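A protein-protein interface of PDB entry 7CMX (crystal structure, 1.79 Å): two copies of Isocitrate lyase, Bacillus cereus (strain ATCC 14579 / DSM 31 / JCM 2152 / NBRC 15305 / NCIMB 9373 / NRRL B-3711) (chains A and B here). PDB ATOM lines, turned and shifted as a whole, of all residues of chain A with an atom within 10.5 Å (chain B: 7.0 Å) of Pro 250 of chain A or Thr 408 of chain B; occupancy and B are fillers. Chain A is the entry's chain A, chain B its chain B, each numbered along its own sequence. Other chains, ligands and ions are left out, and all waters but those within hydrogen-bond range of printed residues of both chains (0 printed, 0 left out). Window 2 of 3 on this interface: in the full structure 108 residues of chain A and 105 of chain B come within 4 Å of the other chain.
The side-chain hydroxyl (OG1) of Thr 249 of chain A is in hydrogen-bond range of the backbone NH (N) of Phe 253 of chain A, 3.1 Å away.
The side-chain hydroxyl of Thr 249 of chain A sits at hydrogen-bond distance from the side-chain carboxylate of Glu 251 of chain A (2.8 Å).
OG1 of Thr 249 of chain A lies within hydrogen-bond range of N of Gly 252 of chain A (3.4 Å).
The side-chain hydroxyl (OG1) of Thr 405 of chain B is in hydrogen-bond range of the backbone NH (N) of Ser 409 of chain B (3.1 Å).
OG of Ser 409 of chain B is in hydrogen-bond range of N of Thr 411 of chain B (3.1 Å).
The side-chain hydroxyl of Thr 408 of chain B is in hydrogen-bond range of the backbone carbonyl oxygen of Thr 405 of chain B (2.6 Å).
No position is printed for both chains.
Of the printed residues of chain B, Glu 183 of chain A touches Thr 411 (2.7 Å).
Of the printed residues of chain B, Thr 249 of chain A touches Ser 410.
Printed residues of chain B within 4 Å of Glu 251 of chain A: Ser 409 (3.5 Å) and Ser 410 (2.7 Å).
Printed residues of chain B within 4 Å of Phe 253 of chain A: Thr 411.
No residue of chain A comes within 4 Å of Gly 406 of chain B.
No residue of chain A comes within 4 Å of Gly 407 of chain B.
Of chain A, only Pro 250 comes within 4 Å of Thr 408 of chain B.
Ser 409 of chain B touches just one residue of chain A: Glu 251 (3.5 Å).
Of the printed residues of chain A, Ser 410 of chain B touches Thr 249 and Glu 251.
The nearest residue of chain A that does not touch Thr 408 of chain B is Glu 251 of chain A (4.1 Å).
The nearest printed residue of chain B that does not touch Glu 251 of chain A is Thr 408 of chain B (4.1 Å).
The side-chain carboxylate (OE1) of Glu 251 of chain A lies within hydrogen-bond range of the side-chain hydroxyl (OG) of Ser 410 of chain B (2.7 Å).
The side-chain hydroxyl (OG1) of Thr 411 of chain B lies within hydrogen-bond range of the side-chain carboxylate (OE1) of Glu 183 of chain A, at 2.7 Å.
Of the 14 printed residues of chain A, 5 touch a printed residue of chain B.
Among the printed residues, no Asp or Glu carboxylate lies within 4 Å of a Lys or Arg side-chain nitrogen of the other chain.
Among the printed residues, merely in contact across the chains: Thr 249 of chain A with Ser 410 of chain B (3.4 Å), Pro 250 of chain A with Thr 408 of chain B (3.7 Å), Glu 251 of chain A with Ser 409 of chain B (3.5 Å) and Phe 253 of chain A with Thr 411 of chain B (3.6 Å).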
ATOM      1  N   GLU A 183      -6.049  13.513  24.732  1.00  0.00           N
ATOM      2  CA  GLU A 183      -6.312  14.298  25.974  1.00  0.00           C
ATOM      3  C   GLU A 183      -6.421  13.378  27.205  1.00  0.00           C
ATOM      4  O   GLU A 183      -6.878  13.858  28.268  1.00  0.00           O
ATOM      5  CB  GLU A 183      -7.574  15.145  25.792  1.00  0.00           C
ATOM      6  CG  GLU A 183      -7.437  16.240  24.748  1.00  0.00           C
ATOM      7  CD  GLU A 183      -6.349  17.277  25.013  1.00  0.00           C
ATOM      8  OE1 GLU A 183      -6.244  17.781  26.153  1.00  0.00           O
ATOM      9  OE2 GLU A 183      -5.602  17.584  24.077  1.00  0.00           O
ATOM     10  N   LEU A 231     -16.739  17.061  29.391  1.00  0.00           N
ATOM     11  CA  LEU A 231     -16.399  17.392  27.991  1.00  0.00           C
ATOM     12  C   LEU A 231     -16.523  16.120  27.152  1.00  0.00           C
ATOM     13  O   LEU A 231     -16.212  15.022  27.699  1.00  0.00           O
ATOM     14  CB  LEU A 231     -14.974  17.939  27.918  1.00  0.00           C
ATOM     15  CG  LEU A 231     -14.736  19.289  28.577  1.00  0.00           C
ATOM     16  CD1 LEU A 231     -13.243  19.575  28.646  1.00  0.00           C
ATOM     17  CD2 LEU A 231     -15.491  20.410  27.847  1.00  0.00           C
ATOM     18  N   ILE A 232     -16.932  16.306  25.896  1.00  0.00           N
ATOM     19  CA  ILE A 232     -17.047  15.264  24.844  1.00  0.00           C
ATOM     20  C   ILE A 232     -16.471  15.846  23.549  1.00  0.00           C
ATOM     21  O   ILE A 232     -16.495  17.093  23.385  1.00  0.00           O
ATOM     22  CB  ILE A 232     -18.509  14.783  24.742  1.00  0.00           C
ATOM     23  CG1 ILE A 232     -18.622  13.433  24.036  1.00  0.00           C
ATOM     24  CG2 ILE A 232     -19.402  15.818  24.084  1.00  0.00           C
ATOM     25  CD1 ILE A 232     -20.061  12.964  23.904  1.00  0.00           C
ATOM     26  N   THR A 233     -15.917  14.995  22.684  1.00  0.00           N
ATOM     27  CA  THR A 233     -15.143  15.439  21.505  1.00  0.00           C
ATOM     28  C   THR A 233     -16.121  16.083  20.532  1.00  0.00           C
ATOM     29  O   THR A 233     -15.730  17.037  19.854  1.00  0.00           O
ATOM     30  CB  THR A 233     -14.349  14.317  20.821  1.00  0.00           C
ATOM     31  OG1 THR A 233     -15.260  13.283  20.465  1.00  0.00           O
ATOM     32  CG2 THR A 233     -13.273  13.691  21.682  1.00  0.00           C
ATOM     33  N   GLY A 246     -24.444  22.389  24.572  1.00  0.00           N
ATOM     34  CA  GLY A 246     -24.315  23.271  23.402  1.00  0.00           C
ATOM     35  C   GLY A 246     -23.170  24.251  23.572  1.00  0.00           C
ATOM     36  O   GLY A 246     -22.735  24.844  22.568  1.00  0.00           O
ATOM     37  N   GLU A 247     -22.658  24.409  24.788  1.00  0.00           N
ATOM     38  CA  GLU A 247     -21.470  25.260  25.017  1.00  0.00           C
ATOM     39  C   GLU A 247     -20.268  24.518  24.430  1.00  0.00           C
ATOM     40  O   GLU A 247     -20.242  23.260  24.501  1.00  0.00           O
ATOM     41  CB  GLU A 247     -21.263  25.596  26.493  1.00  0.00           C
ATOM     42  CG  GLU A 247     -22.539  25.992  27.220  1.00  0.00           C
ATOM     43  CD  GLU A 247     -22.436  25.853  28.734  1.00  0.00           C
ATOM     44  OE1 GLU A 247     -22.423  24.695  29.248  1.00  0.00           O
ATOM     45  OE2 GLU A 247     -22.314  26.908  29.395  1.00  0.00           O
ATOM     46  N   ARG A 248     -19.308  25.259  23.880  1.00  0.00           N
ATOM     47  CA  ARG A 248     -18.050  24.687  23.335  1.00  0.00           C
ATOM     48  C   ARG A 248     -16.840  25.386  23.943  1.00  0.00           C
ATOM     49  O   ARG A 248     -16.977  26.557  24.332  1.00  0.00           O
ATOM     50  CB  ARG A 248     -18.072  24.757  21.810  1.00  0.00           C
ATOM     51  CG  ARG A 248     -19.154  23.860  21.236  1.00  0.00           C
ATOM     52  CD  ARG A 248     -19.078  23.721  19.755  1.00  0.00           C
ATOM     53  NE  ARG A 248     -17.932  22.943  19.365  1.00  0.00           N
ATOM     54  CZ  ARG A 248     -17.538  22.795  18.110  1.00  0.00           C
ATOM     55  NH1 ARG A 248     -18.199  23.392  17.141  1.00  0.00           N
ATOM     56  NH2 ARG A 248     -16.489  22.053  17.809  1.00  0.00           N
ATOM     57  N   THR A 249     -15.714  24.659  24.047  1.00  0.00           N
ATOM     58  CA  THR A 249     -14.421  25.138  24.601  1.00  0.00           C
ATOM     59  C   THR A 249     -13.639  25.781  23.469  1.00  0.00           C
ATOM     60  O   THR A 249     -14.019  25.610  22.313  1.00  0.00           O
ATOM     61  CB  THR A 249     -13.637  23.983  25.243  1.00  0.00           C
ATOM     62  OG1 THR A 249     -13.202  23.074  24.227  1.00  0.00           O
ATOM     63  CG2 THR A 249     -14.462  23.262  26.287  1.00  0.00           C
ATOM     64  N   PRO A 250     -12.517  26.502  23.733  1.00  0.00           N
ATOM     65  CA  PRO A 250     -11.716  27.061  22.640  1.00  0.00           C
ATOM     66  C   PRO A 250     -11.206  26.023  21.632  1.00  0.00           C
ATOM     67  O   PRO A 250     -11.072  26.372  20.457  1.00  0.00           O
ATOM     68  CB  PRO A 250     -10.582  27.783  23.375  1.00  0.00           C
ATOM     69  CG  PRO A 250     -11.253  28.214  24.652  1.00  0.00           C
ATOM     70  CD  PRO A 250     -12.034  26.960  25.043  1.00  0.00           C
ATOM     71  N   GLU A 251     -10.959  24.792  22.100  1.00  0.00           N
ATOM     72  CA  GLU A 251     -10.467  23.650  21.292  1.00  0.00           C
ATOM     73  C   GLU A 251     -11.613  23.056  20.483  1.00  0.00           C
ATOM     74  O   GLU A 251     -11.329  22.327  19.521  1.00  0.00           O
ATOM     75  CB  GLU A 251      -9.957  22.493  22.157  1.00  0.00           C
ATOM     76  CG  GLU A 251      -8.829  22.862  23.094  1.00  0.00           C
ATOM     77  CD  GLU A 251      -9.307  23.264  24.476  1.00  0.00           C
ATOM     78  OE1 GLU A 251     -10.503  23.613  24.619  1.00  0.00           O
ATOM     79  OE2 GLU A 251      -8.471  23.260  25.411  1.00  0.00           O
ATOM     80  N   GLY A 252     -12.863  23.284  20.891  1.00  0.00           N
ATOM     81  CA  GLY A 252     -14.024  22.787  20.123  1.00  0.00           C
ATOM     82  C   GLY A 252     -14.685  21.598  20.781  1.00  0.00           C
ATOM     83  O   GLY A 252     -15.673  21.104  20.233  1.00  0.00           O
ATOM     84  N   PHE A 253     -14.240  21.199  21.970  1.00  0.00           N
ATOM     85  CA  PHE A 253     -14.950  20.179  22.779  1.00  0.00           C
ATOM     86  C   PHE A 253     -16.335  20.712  23.188  1.00  0.00           C
ATOM     87  O   PHE A 253     -16.506  21.914  23.365  1.00  0.00           O
ATOM     88  CB  PHE A 253     -14.103  19.780  23.987  1.00  0.00           C
ATOM     89  CG  PHE A 253     -12.711  19.340  23.642  1.00  0.00           C
ATOM     90  CD1 PHE A 253     -12.483  18.477  22.587  1.00  0.00           C
ATOM     91  CD2 PHE A 253     -11.629  19.764  24.391  1.00  0.00           C
ATOM     92  CE1 PHE A 253     -11.199  18.062  22.268  1.00  0.00           C
ATOM     93  CE2 PHE A 253     -10.349  19.329  24.085  1.00  0.00           C
ATOM     94  CZ  PHE A 253     -10.137  18.472  23.032  1.00  0.00           C
ATOM     95  N   TYR A 254     -17.304  19.831  23.381  1.00  0.00           N
ATOM     96  CA  TYR A 254     -18.676  20.185  23.837  1.00  0.00           C
ATOM     97  C   TYR A 254     -18.795  19.904  25.337  1.00  0.00           C
ATOM     98  O   TYR A 254     -18.384  18.824  25.833  1.00  0.00           O
ATOM     99  CB  TYR A 254     -19.721  19.388  23.059  1.00  0.00           C
ATOM    100  CG  TYR A 254     -19.777  19.687  21.588  1.00  0.00           C
ATOM    101  CD1 TYR A 254     -18.756  19.308  20.735  1.00  0.00           C
ATOM    102  CD2 TYR A 254     -20.877  20.327  21.045  1.00  0.00           C
ATOM    103  CE1 TYR A 254     -18.828  19.554  19.370  1.00  0.00           C
ATOM    104  CE2 TYR A 254     -20.979  20.550  19.683  1.00  0.00           C
ATOM    105  CZ  TYR A 254     -19.942  20.174  18.851  1.00  0.00           C
ATOM    106  OH  TYR A 254     -20.009  20.467  17.530  1.00  0.00           O
ATOM    107  N   ARG A 255     -19.344  20.865  26.070  1.00  0.00           N
ATOM    108  CA  ARG A 255     -19.569  20.710  27.523  1.00  0.00           C
ATOM    109  C   ARG A 255     -20.752  19.758  27.689  1.00  0.00           C
ATOM    110  O   ARG A 255     -21.697  19.799  26.844  1.00  0.00           O
ATOM    111  CB  ARG A 255     -19.803  22.060  28.196  1.00  0.00           C
ATOM    112  CG  ARG A 255     -18.761  23.110  27.834  1.00  0.00           C
ATOM    113  CD  ARG A 255     -18.623  24.234  28.859  1.00  0.00           C
ATOM    114  NE  ARG A 255     -17.588  23.744  29.739  1.00  0.00           N
ATOM    115  CZ  ARG A 255     -16.353  24.212  29.810  1.00  0.00           C
ATOM    116  NH1 ARG A 255     -15.983  25.294  29.149  1.00  0.00           N
ATOM    117  NH2 ARG A 255     -15.505  23.621  30.618  1.00  0.00           N
ATOM    118  N   ALA B 401       1.306  23.012  28.928  1.00  0.00           N
ATOM    119  CA  ALA B 401       0.040  23.115  28.152  1.00  0.00           C
ATOM    120  C   ALA B 401      -0.448  24.573  28.105  1.00  0.00           C
ATOM    121  O   ALA B 401      -0.891  25.012  27.037  1.00  0.00           O
ATOM    122  CB  ALA B 401      -1.015  22.215  28.723  1.00  0.00           C
ATOM    123  N   GLN B 402      -0.419  25.286  29.233  1.00  0.00           N
ATOM    124  CA  GLN B 402      -0.842  26.719  29.324  1.00  0.00           C
ATOM    125  C   GLN B 402       0.108  27.597  28.499  1.00  0.00           C
ATOM    126  O   GLN B 402      -0.363  28.492  27.777  1.00  0.00           O
ATOM    127  CB  GLN B 402      -0.911  27.182  30.781  1.00  0.00           C
ATOM    128  CG  GLN B 402      -2.007  26.494  31.580  1.00  0.00           C
ATOM    129  CD  GLN B 402      -3.386  26.942  31.161  1.00  0.00           C
ATOM    130  OE1 GLN B 402      -3.696  27.083  29.980  1.00  0.00           O
ATOM    131  NE2 GLN B 402      -4.263  27.137  32.118  1.00  0.00           N
ATOM    132  N   ILE B 404       1.853  26.617  25.777  1.00  0.00           N
ATOM    133  CA  ILE B 404       1.591  26.312  24.340  1.00  0.00           C
ATOM    134  C   ILE B 404       0.292  27.033  23.906  1.00  0.00           C
ATOM    135  O   ILE B 404       0.240  27.535  22.774  1.00  0.00           O
ATOM    136  CB  ILE B 404       1.490  24.790  24.122  1.00  0.00           C
ATOM    137  CG1 ILE B 404       2.831  24.093  24.350  1.00  0.00           C
ATOM    138  CG2 ILE B 404       0.902  24.460  22.748  1.00  0.00           C
ATOM    139  CD1 ILE B 404       2.719  22.593  24.628  1.00  0.00           C
ATOM    140  N   THR B 405      -0.751  26.990  24.745  1.00  0.00           N
ATOM    141  CA  THR B 405      -2.132  27.441  24.398  1.00  0.00           C
ATOM    142  C   THR B 405      -2.336  28.921  24.742  1.00  0.00           C
ATOM    143  O   THR B 405      -3.438  29.382  24.501  1.00  0.00           O
ATOM    144  CB  THR B 405      -3.216  26.563  25.042  1.00  0.00           C
ATOM    145  OG1 THR B 405      -3.187  26.713  26.462  1.00  0.00           O
ATOM    146  CG2 THR B 405      -3.082  25.104  24.660  1.00  0.00           C
ATOM    147  N   GLY B 406      -1.310  29.671  25.149  1.00  0.00           N
ATOM    148  CA  GLY B 406      -1.453  31.078  25.585  1.00  0.00           C
ATOM    149  C   GLY B 406      -2.478  31.212  26.710  1.00  0.00           C
ATOM    150  O   GLY B 406      -3.245  32.217  26.735  1.00  0.00           O
ATOM    151  N   GLY B 407      -2.584  30.192  27.564  1.00  0.00           N
ATOM    152  CA  GLY B 407      -3.507  30.216  28.706  1.00  0.00           C
ATOM    153  C   GLY B 407      -4.941  29.856  28.368  1.00  0.00           C
ATOM    154  O   GLY B 407      -5.774  30.088  29.264  1.00  0.00           O
ATOM    155  N   THR B 408      -5.227  29.284  27.178  1.00  0.00           N
ATOM    156  CA  THR B 408      -6.614  29.011  26.717  1.00  0.00           C
ATOM    157  C   THR B 408      -7.020  27.532  26.866  1.00  0.00           C
ATOM    158  O   THR B 408      -8.155  27.225  26.516  1.00  0.00           O
ATOM    159  CB  THR B 408      -6.826  29.469  25.277  1.00  0.00           C
ATOM    160  OG1 THR B 408      -5.943  28.670  24.487  1.00  0.00           O
ATOM    161  CG2 THR B 408      -6.574  30.956  25.110  1.00  0.00           C
ATOM    162  N   SER B 409      -6.159  26.650  27.366  1.00  0.00           N
ATOM    163  CA  SER B 409      -6.473  25.202  27.484  1.00  0.00           C
ATOM    164  C   SER B 409      -7.669  25.008  28.430  1.00  0.00           C
ATOM    165  O   SER B 409      -7.699  25.586  29.530  1.00  0.00           O
ATOM    166  CB  SER B 409      -5.266  24.383  27.955  1.00  0.00           C
ATOM    167  OG  SER B 409      -5.715  23.097  28.354  1.00  0.00           O
ATOM    168  N   SER B 410      -8.625  24.183  28.044  1.00  0.00           N
ATOM    169  CA  SER B 410      -9.753  23.818  28.940  1.00  0.00           C
ATOM    170  C   SER B 410      -9.492  22.439  29.563  1.00  0.00           C
ATOM    171  O   SER B 410     -10.367  21.982  30.304  1.00  0.00           O
ATOM    172  CB  SER B 410     -11.072  23.846  28.204  1.00  0.00           C
ATOM    173  OG  SER B 410     -11.078  22.882  27.163  1.00  0.00           O
ATOM    174  N   THR B 411      -8.349  21.798  29.290  1.00  0.00           N
ATOM    175  CA  THR B 411      -8.080  20.379  29.679  1.00  0.00           C
ATOM    176  C   THR B 411      -6.858  20.238  30.599  1.00  0.00           C
ATOM    177  O   THR B 411      -6.191  19.174  30.527  1.00  0.00           O
ATOM    178  CB  THR B 411      -7.879  19.511  28.435  1.00  0.00           C
ATOM    179  OG1 THR B 411      -6.693  19.948  27.766  1.00  0.00           O
ATOM    180  CG2 THR B 411      -9.059  19.571  27.487  1.00  0.00           C
